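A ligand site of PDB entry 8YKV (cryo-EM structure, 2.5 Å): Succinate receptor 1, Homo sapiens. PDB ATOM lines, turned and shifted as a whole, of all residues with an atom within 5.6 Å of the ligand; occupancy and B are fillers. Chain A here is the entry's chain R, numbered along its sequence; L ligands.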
ATOM      1  N   GLU A  22      -5.593  -1.492   3.246  1.00  0.00           N
ATOM      2  CA  GLU A  22      -6.819  -2.143   3.678  1.00  0.00           C
ATOM      3  C   GLU A  22      -8.056  -1.462   3.097  1.00  0.00           C
ATOM      4  O   GLU A  22      -9.008  -2.130   2.684  1.00  0.00           O
ATOM      5  CB  GLU A  22      -6.904  -2.162   5.203  1.00  0.00           C
ATOM      6  CG  GLU A  22      -6.031  -3.233   5.855  1.00  0.00           C
ATOM      7  CD  GLU A  22      -6.370  -3.449   7.320  1.00  0.00           C
ATOM      8  OE1 GLU A  22      -6.796  -2.484   7.984  1.00  0.00           O
ATOM      9  OE2 GLU A  22      -6.209  -4.587   7.800  1.00  0.00           O
ATOM     10  N   LEU A  26      -7.622  -2.689  -1.326  1.00  0.00           N
ATOM     11  CA  LEU A  26      -8.495  -3.854  -1.319  1.00  0.00           C
ATOM     12  C   LEU A  26      -9.822  -3.541  -2.002  1.00  0.00           C
ATOM     13  O   LEU A  26     -10.247  -4.258  -2.919  1.00  0.00           O
ATOM     14  CB  LEU A  26      -8.734  -4.334   0.118  1.00  0.00           C
ATOM     15  CG  LEU A  26      -7.584  -5.072   0.814  1.00  0.00           C
ATOM     16  CD1 LEU A  26      -7.966  -5.395   2.254  1.00  0.00           C
ATOM     17  CD2 LEU A  26      -7.206  -6.344   0.069  1.00  0.00           C
ATOM     18  N   TYR A  30     -10.535  -5.279  -5.589  1.00  0.00           N
ATOM     19  CA  TYR A  30     -11.629  -6.239  -5.568  1.00  0.00           C
ATOM     20  C   TYR A  30     -12.780  -5.800  -6.447  1.00  0.00           C
ATOM     21  O   TYR A  30     -13.389  -6.630  -7.124  1.00  0.00           O
ATOM     22  CB  TYR A  30     -12.122  -6.444  -4.136  1.00  0.00           C
ATOM     23  CG  TYR A  30     -11.313  -7.403  -3.299  1.00  0.00           C
ATOM     24  CD1 TYR A  30     -10.005  -7.115  -2.943  1.00  0.00           C
ATOM     25  CD2 TYR A  30     -11.883  -8.575  -2.824  1.00  0.00           C
ATOM     26  CE1 TYR A  30      -9.274  -7.983  -2.169  1.00  0.00           C
ATOM     27  CE2 TYR A  30     -11.160  -9.454  -2.048  1.00  0.00           C
ATOM     28  CZ  TYR A  30      -9.855  -9.150  -1.721  1.00  0.00           C
ATOM     29  OH  TYR A  30      -9.117 -10.013  -0.940  1.00  0.00           O
ATOM     30  N   THR A  75     -19.145 -13.175  -3.742  1.00  0.00           N
ATOM     31  CA  THR A  75     -18.865 -12.887  -2.342  1.00  0.00           C
ATOM     32  C   THR A  75     -17.989 -11.656  -2.152  1.00  0.00           C
ATOM     33  O   THR A  75     -17.676 -11.307  -1.003  1.00  0.00           O
ATOM     34  CB  THR A  75     -18.172 -14.094  -1.679  1.00  0.00           C
ATOM     35  OG1 THR A  75     -16.761 -14.029  -1.919  1.00  0.00           O
ATOM     36  CG2 THR A  75     -18.725 -15.404  -2.226  1.00  0.00           C
ATOM     37  N   MET A  78     -19.769  -7.500  -0.834  1.00  0.00           N
ATOM     38  CA  MET A  78     -20.002  -7.210   0.575  1.00  0.00           C
ATOM     39  C   MET A  78     -18.707  -6.737   1.249  1.00  0.00           C
ATOM     40  O   MET A  78     -18.687  -5.698   1.911  1.00  0.00           O
ATOM     41  CB  MET A  78     -20.537  -8.455   1.283  1.00  0.00           C
ATOM     42  CG  MET A  78     -21.992  -8.752   0.972  1.00  0.00           C
ATOM     43  SD  MET A  78     -22.542 -10.322   1.666  1.00  0.00           S
ATOM     44  CE  MET A  78     -22.139 -11.445   0.331  1.00  0.00           C
ATOM     45  N   LEU A  79     -17.641  -7.522   1.079  1.00  0.00           N
ATOM     46  CA  LEU A  79     -16.349  -7.163   1.665  1.00  0.00           C
ATOM     47  C   LEU A  79     -15.770  -5.920   0.999  1.00  0.00           C
ATOM     48  O   LEU A  79     -15.033  -5.247   1.654  1.00  0.00           O
ATOM     49  CB  LEU A  79     -15.364  -8.336   1.600  1.00  0.00           C
ATOM     50  CG  LEU A  79     -14.894  -8.914   0.257  1.00  0.00           C
ATOM     51  CD1 LEU A  79     -13.770  -8.099  -0.315  1.00  0.00           C
ATOM     52  CD2 LEU A  79     -14.539 -10.388   0.360  1.00  0.00           C
ATOM     53  N   SER A  82     -17.441  -3.198   2.823  1.00  0.00           N
ATOM     54  CA  SER A  82     -16.917  -3.158   4.178  1.00  0.00           C
ATOM     55  C   SER A  82     -15.528  -2.509   4.208  1.00  0.00           C
ATOM     56  O   SER A  82     -15.247  -1.678   5.087  1.00  0.00           O
ATOM     57  CB  SER A  82     -16.860  -4.573   4.763  1.00  0.00           C
ATOM     58  OG  SER A  82     -18.137  -5.167   4.728  1.00  0.00           O
ATOM     59  N   TYR A  83     -14.634  -2.870   3.277  1.00  0.00           N
ATOM     60  CA  TYR A  83     -13.307  -2.254   3.246  1.00  0.00           C
ATOM     61  C   TYR A  83     -13.400  -0.775   2.980  1.00  0.00           C
ATOM     62  O   TYR A  83     -12.699   0.012   3.629  1.00  0.00           O
ATOM     63  CB  TYR A  83     -12.364  -2.896   2.203  1.00  0.00           C
ATOM     64  CG  TYR A  83     -11.889  -4.260   2.620  1.00  0.00           C
ATOM     65  CD1 TYR A  83     -11.278  -4.471   3.848  1.00  0.00           C
ATOM     66  CD2 TYR A  83     -12.058  -5.354   1.782  1.00  0.00           C
ATOM     67  CE1 TYR A  83     -10.870  -5.709   4.243  1.00  0.00           C
ATOM     68  CE2 TYR A  83     -11.648  -6.603   2.170  1.00  0.00           C
ATOM     69  CZ  TYR A  83     -11.052  -6.772   3.407  1.00  0.00           C
ATOM     70  OH  TYR A  83     -10.608  -7.975   3.851  1.00  0.00           O
ATOM     71  N   GLY A  86     -14.766   0.449   6.125  1.00  0.00           N
ATOM     72  CA  GLY A  86     -13.936   0.077   7.253  1.00  0.00           C
ATOM     73  C   GLY A  86     -14.636  -0.720   8.323  1.00  0.00           C
ATOM     74  O   GLY A  86     -14.078  -0.881   9.423  1.00  0.00           O
ATOM     75  N   ASN A  87     -15.827  -1.239   8.057  1.00  0.00           N
ATOM     76  CA  ASN A  87     -16.556  -2.026   9.045  1.00  0.00           C
ATOM     77  C   ASN A  87     -17.500  -2.977   8.311  1.00  0.00           C
ATOM     78  O   ASN A  87     -17.893  -2.709   7.175  1.00  0.00           O
ATOM     79  CB  ASN A  87     -17.329  -1.111  10.009  1.00  0.00           C
ATOM     80  CG  ASN A  87     -17.864  -1.845  11.230  1.00  0.00           C
ATOM     81  OD1 ASN A  87     -17.275  -2.820  11.708  1.00  0.00           O
ATOM     82  ND2 ASN A  87     -19.005  -1.386  11.738  1.00  0.00           N
ATOM     83  N   TRP A  88     -17.847  -4.071   8.970  1.00  0.00           N
ATOM     84  CA  TRP A  88     -18.760  -5.056   8.404  1.00  0.00           C
ATOM     85  C   TRP A  88     -20.183  -4.700   8.839  1.00  0.00           C
ATOM     86  O   TRP A  88     -20.471  -4.631  10.042  1.00  0.00           O
ATOM     87  CB  TRP A  88     -18.378  -6.457   8.859  1.00  0.00           C
ATOM     88  CG  TRP A  88     -19.283  -7.551   8.353  1.00  0.00           C
ATOM     89  CD1 TRP A  88     -20.218  -8.229   9.069  1.00  0.00           C
ATOM     90  CD2 TRP A  88     -19.324  -8.081   7.024  1.00  0.00           C
ATOM     91  NE1 TRP A  88     -20.847  -9.156   8.269  1.00  0.00           N
ATOM     92  CE2 TRP A  88     -20.315  -9.086   7.008  1.00  0.00           C
ATOM     93  CE3 TRP A  88     -18.629  -7.817   5.845  1.00  0.00           C
ATOM     94  CZ2 TRP A  88     -20.623  -9.817   5.865  1.00  0.00           C
ATOM     95  CZ3 TRP A  88     -18.939  -8.536   4.708  1.00  0.00           C
ATOM     96  CH2 TRP A  88     -19.928  -9.528   4.728  1.00  0.00           C
ATOM     97  N   CYS A  95     -21.480 -12.865   7.504  1.00  0.00           N
ATOM     98  CA  CYS A  95     -20.022 -12.941   7.534  1.00  0.00           C
ATOM     99  C   CYS A  95     -19.558 -14.388   7.397  1.00  0.00           C
ATOM    100  O   CYS A  95     -18.694 -14.706   6.570  1.00  0.00           O
ATOM    101  CB  CYS A  95     -19.490 -12.324   8.825  1.00  0.00           C
ATOM    102  SG  CYS A  95     -17.688 -12.222   8.916  1.00  0.00           S
ATOM    103  N   ASN A  98     -20.352 -15.772   3.918  1.00  0.00           N
ATOM    104  CA  ASN A  98     -19.484 -15.219   2.888  1.00  0.00           C
ATOM    105  C   ASN A  98     -18.106 -15.843   2.957  1.00  0.00           C
ATOM    106  O   ASN A  98     -17.551 -16.228   1.915  1.00  0.00           O
ATOM    107  CB  ASN A  98     -19.394 -13.699   3.056  1.00  0.00           C
ATOM    108  CG  ASN A  98     -19.197 -12.977   1.746  1.00  0.00           C
ATOM    109  OD1 ASN A  98     -19.884 -13.264   0.769  1.00  0.00           O
ATOM    110  ND2 ASN A  98     -18.263 -12.033   1.723  1.00  0.00           N
ATOM    111  N   ARG A  99     -17.555 -15.981   4.157  1.00  0.00           N
ATOM    112  CA  ARG A  99     -16.254 -16.618   4.324  1.00  0.00           C
ATOM    113  C   ARG A  99     -16.291 -18.012   3.727  1.00  0.00           C
ATOM    114  O   ARG A  99     -15.431 -18.369   2.923  1.00  0.00           O
ATOM    115  CB  ARG A  99     -15.952 -16.721   5.820  1.00  0.00           C
ATOM    116  CG  ARG A  99     -14.493 -16.816   6.195  1.00  0.00           C
ATOM    117  CD  ARG A  99     -14.329 -16.989   7.700  1.00  0.00           C
ATOM    118  NE  ARG A  99     -14.354 -15.717   8.419  1.00  0.00           N
ATOM    119  CZ  ARG A  99     -15.244 -15.415   9.351  1.00  0.00           C
ATOM    120  NH1 ARG A  99     -16.191 -16.279   9.675  1.00  0.00           N
ATOM    121  NH2 ARG A  99     -15.195 -14.241   9.962  1.00  0.00           N
ATOM    122  N   LEU A 102     -16.709 -18.055  -0.174  1.00  0.00           N
ATOM    123  CA  LEU A 102     -15.483 -17.576  -0.807  1.00  0.00           C
ATOM    124  C   LEU A 102     -14.431 -18.672  -0.856  1.00  0.00           C
ATOM    125  O   LEU A 102     -13.961 -19.028  -1.928  1.00  0.00           O
ATOM    126  CB  LEU A 102     -14.908 -16.384  -0.023  1.00  0.00           C
ATOM    127  CG  LEU A 102     -13.820 -15.506  -0.670  1.00  0.00           C
ATOM    128  CD1 LEU A 102     -13.962 -14.043  -0.283  1.00  0.00           C
ATOM    129  CD2 LEU A 102     -12.408 -15.996  -0.410  1.00  0.00           C
ATOM    130  N   HIS A 103     -14.071 -19.214   0.303  1.00  0.00           N
ATOM    131  CA  HIS A 103     -12.977 -20.182   0.343  1.00  0.00           C
ATOM    132  C   HIS A 103     -13.353 -21.474  -0.383  1.00  0.00           C
ATOM    133  O   HIS A 103     -12.523 -22.068  -1.088  1.00  0.00           O
ATOM    134  CB  HIS A 103     -12.590 -20.457   1.788  1.00  0.00           C
ATOM    135  CG  HIS A 103     -12.004 -19.271   2.485  1.00  0.00           C
ATOM    136  ND1 HIS A 103     -10.816 -18.684   2.083  1.00  0.00           N
ATOM    137  CD2 HIS A 103     -12.432 -18.553   3.545  1.00  0.00           C
ATOM    138  CE1 HIS A 103     -10.542 -17.660   2.870  1.00  0.00           C
ATOM    139  NE2 HIS A 103     -11.506 -17.562   3.764  1.00  0.00           N
ATOM    140  N   ASP A 174     -12.786 -12.662   8.257  1.00  0.00           N
ATOM    141  CA  ASP A 174     -11.516 -12.630   7.554  1.00  0.00           C
ATOM    142  C   ASP A 174     -10.802 -13.802   8.034  1.00  0.00           C
ATOM    143  O   ASP A 174     -10.153 -13.736   9.054  1.00  0.00           O
ATOM    144  CB  ASP A 174     -10.734 -11.344   7.879  1.00  0.00           C
ATOM    145  CG  ASP A 174      -9.255 -11.356   7.338  1.00  0.00           C
ATOM    146  OD1 ASP A 174      -8.824 -12.256   6.592  1.00  0.00           O
ATOM    147  OD2 ASP A 174      -8.514 -10.414   7.675  1.00  0.00           O
ATOM    148  N   PHE A 175     -10.929 -14.915   7.341  1.00  0.00           N
ATOM    149  CA  PHE A 175     -10.329 -16.145   7.848  1.00  0.00           C
ATOM    150  C   PHE A 175      -8.985 -16.048   8.628  1.00  0.00           C
ATOM    151  O   PHE A 175      -8.946 -16.467   9.754  1.00  0.00           O
ATOM    152  CB  PHE A 175     -10.247 -17.185   6.747  1.00  0.00           C
ATOM    153  CG  PHE A 175      -9.560 -18.438   7.162  1.00  0.00           C
ATOM    154  CD1 PHE A 175     -10.217 -19.382   7.901  1.00  0.00           C
ATOM    155  CD2 PHE A 175      -8.245 -18.659   6.833  1.00  0.00           C
ATOM    156  CE1 PHE A 175      -9.582 -20.539   8.293  1.00  0.00           C
ATOM    157  CE2 PHE A 175      -7.591 -19.807   7.214  1.00  0.00           C
ATOM    158  CZ  PHE A 175      -8.261 -20.750   7.948  1.00  0.00           C
ATOM    159  N   TYR A 248      -0.290 -16.160  -2.019  1.00  0.00           N
ATOM    160  CA  TYR A 248      -1.428 -16.019  -1.121  1.00  0.00           C
ATOM    161  C   TYR A 248      -1.458 -17.139  -0.088  1.00  0.00           C
ATOM    162  O   TYR A 248      -1.649 -16.892   1.108  1.00  0.00           O
ATOM    163  CB  TYR A 248      -2.722 -16.006  -1.934  1.00  0.00           C
ATOM    164  CG  TYR A 248      -3.964 -16.355  -1.159  1.00  0.00           C
ATOM    165  CD1 TYR A 248      -4.421 -15.544  -0.127  1.00  0.00           C
ATOM    166  CD2 TYR A 248      -4.695 -17.493  -1.455  1.00  0.00           C
ATOM    167  CE1 TYR A 248      -5.553 -15.865   0.586  1.00  0.00           C
ATOM    168  CE2 TYR A 248      -5.839 -17.825  -0.754  1.00  0.00           C
ATOM    169  CZ  TYR A 248      -6.259 -17.000   0.265  1.00  0.00           C
ATOM    170  OH  TYR A 248      -7.398 -17.327   0.972  1.00  0.00           O
ATOM    171  N   ARG A 281      -3.417 -11.209  -1.154  1.00  0.00           N
ATOM    172  CA  ARG A 281      -4.762 -11.775  -1.187  1.00  0.00           C
ATOM    173  C   ARG A 281      -5.511 -11.498  -2.482  1.00  0.00           C
ATOM    174  O   ARG A 281      -6.013 -12.461  -3.086  1.00  0.00           O
ATOM    175  CB  ARG A 281      -5.554 -11.275   0.031  1.00  0.00           C
ATOM    176  CG  ARG A 281      -6.764 -12.141   0.367  1.00  0.00           C
ATOM    177  CD  ARG A 281      -6.947 -12.409   1.853  1.00  0.00           C
ATOM    178  NE  ARG A 281      -7.432 -11.245   2.583  1.00  0.00           N
ATOM    179  CZ  ARG A 281      -6.663 -10.318   3.138  1.00  0.00           C
ATOM    180  NH1 ARG A 281      -5.334 -10.436   3.161  1.00  0.00           N
ATOM    181  NH2 ARG A 281      -7.216  -9.255   3.697  1.00  0.00           N
ATOM    182  N   PHE A 285      -7.212 -14.177  -5.966  1.00  0.00           N
ATOM    183  CA  PHE A 285      -8.584 -14.106  -6.432  1.00  0.00           C
ATOM    184  C   PHE A 285      -8.667 -13.630  -7.883  1.00  0.00           C
ATOM    185  O   PHE A 285      -9.757 -13.674  -8.468  1.00  0.00           O
ATOM    186  CB  PHE A 285      -9.398 -13.185  -5.519  1.00  0.00           C
ATOM    187  CG  PHE A 285      -9.281 -13.530  -4.057  1.00  0.00           C
ATOM    188  CD1 PHE A 285      -9.116 -14.852  -3.657  1.00  0.00           C
ATOM    189  CD2 PHE A 285      -9.352 -12.550  -3.092  1.00  0.00           C
ATOM    190  CE1 PHE A 285      -9.019 -15.173  -2.314  1.00  0.00           C
ATOM    191  CE2 PHE A 285      -9.255 -12.871  -1.749  1.00  0.00           C
ATOM    192  CZ  PHE A 285      -9.083 -14.183  -1.365  1.00  0.00           C
HETATM  193  C1  LIG L   1     -12.531 -13.107   3.519  1.00  0.00           C
HETATM  194  C2  LIG L   1     -12.149 -14.319   2.714  1.00  0.00           C
HETATM  195  C3  LIG L   1     -13.719  -8.084   9.046  1.00  0.00           C
HETATM  196  C4  LIG L   1     -13.587  -6.781   8.621  1.00  0.00           C
HETATM  197  C5  LIG L   1     -13.868  -6.403   7.313  1.00  0.00           C
HETATM  198  C6  LIG L   1     -16.268 -10.520   4.127  1.00  0.00           C
HETATM  199  C7  LIG L   1     -15.834  -9.517   4.968  1.00  0.00           C
HETATM  200  C8  LIG L   1     -14.907  -9.767   5.926  1.00  0.00           C
HETATM  201  N1  LIG L   1     -14.415 -10.955   6.034  1.00  0.00           N
HETATM  202  C9  LIG L   1     -14.811 -11.902   5.220  1.00  0.00           C
HETATM  203  C10 LIG L   1     -15.761 -11.785   4.241  1.00  0.00           C
HETATM  204  C11 LIG L   1     -14.187 -13.221   5.476  1.00  0.00           C
HETATM  205  O1  LIG L   1     -14.601 -13.740   6.419  1.00  0.00           O
HETATM  206  N2  LIG L   1     -13.087 -13.748   4.690  1.00  0.00           N
HETATM  207  C12 LIG L   1     -11.340 -12.161   3.735  1.00  0.00           C
HETATM  208  C13 LIG L   1     -11.155 -11.278   2.500  1.00  0.00           C
HETATM  209  O2  LIG L   1     -10.205 -10.473   2.393  1.00  0.00           O
HETATM  210  O3  LIG L   1     -11.977 -11.356   1.551  1.00  0.00           O
HETATM  211  O4  LIG L   1     -12.936 -15.279   2.764  1.00  0.00           O
HETATM  212  O5  LIG L   1     -11.086 -14.350   2.045  1.00  0.00           O
HETATM  213  C14 LIG L   1     -14.431  -8.682   6.852  1.00  0.00           C
HETATM  214  C15 LIG L   1     -14.149  -9.042   8.159  1.00  0.00           C
HETATM  215  C16 LIG L   1     -14.303  -7.368   6.420  1.00  0.00           C
HETATM  216  O6  LIG L   1     -13.142  -5.822   9.527  1.00  0.00           O
HETATM  217  C17 LIG L   1     -12.535  -4.753   8.900  1.00  0.00           C
HETATM  218  F1  LIG L   1     -12.725  -3.634   9.664  1.00  0.00           F
HETATM  219  F2  LIG L   1     -11.202  -5.012   8.769  1.00  0.00           F
HETATM  220  F3  LIG L   1     -13.103  -4.598   7.666  1.00  0.00           F
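A fluorine (F1) of the ligand sits close to the backbone carbonyl oxygen (O) of Gly 86 (3.1 Å). Merely in contact with the ligand: Leu 79 (3.0 Å), Leu 102 (3.2 Å), Trp 88 (3.3 Å), Asn 98 (3.5 Å), Tyr 30 (3.5 Å), Phe 175 (3.6 Å) and Phe 285 (3.96 Å). Hydrophobic or aromatic side chains that line the ligand: Leu 79, Tyr 83, Trp 88, Leu 102, His 103 and Phe 285. 13 residues have an atom within 4 Å of the ligand: Tyr 30, Leu 79, Tyr 83, Gly 86, Trp 88, Asn 98, Arg 99, Leu 102, His 103, Asp 174, Phe 175, Arg 281 and Phe 285. The nearest printed residue that does not touch the ligand is Ser 82 (4.1 Å).
NH2 of Arg 99 sits at hydrogen-bond distance from SG of Cys 95 (3.4 Å). O of Thr 75 lies within hydrogen-bond range of ND2 of Asn 98, at 2.9 Å.
An oxygen (O1) of the ligand is in hydrogen-bond range of the backbone NH of Asp 174, at 2.8 Å. O1 of the ligand lies within hydrogen-bond range of NE of Arg 99, 2.8 Å away. A ring nitrogen (NE2) of His 103 sits at hydrogen-bond distance from an oxygen (O4) of the ligand. NE of Arg 281 is in salt-bridge range of O2 of the ligand. The side-chain hydroxyl (OH) of Tyr 83 sits at hydrogen-bond distance from an oxygen (O2) of the ligand.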
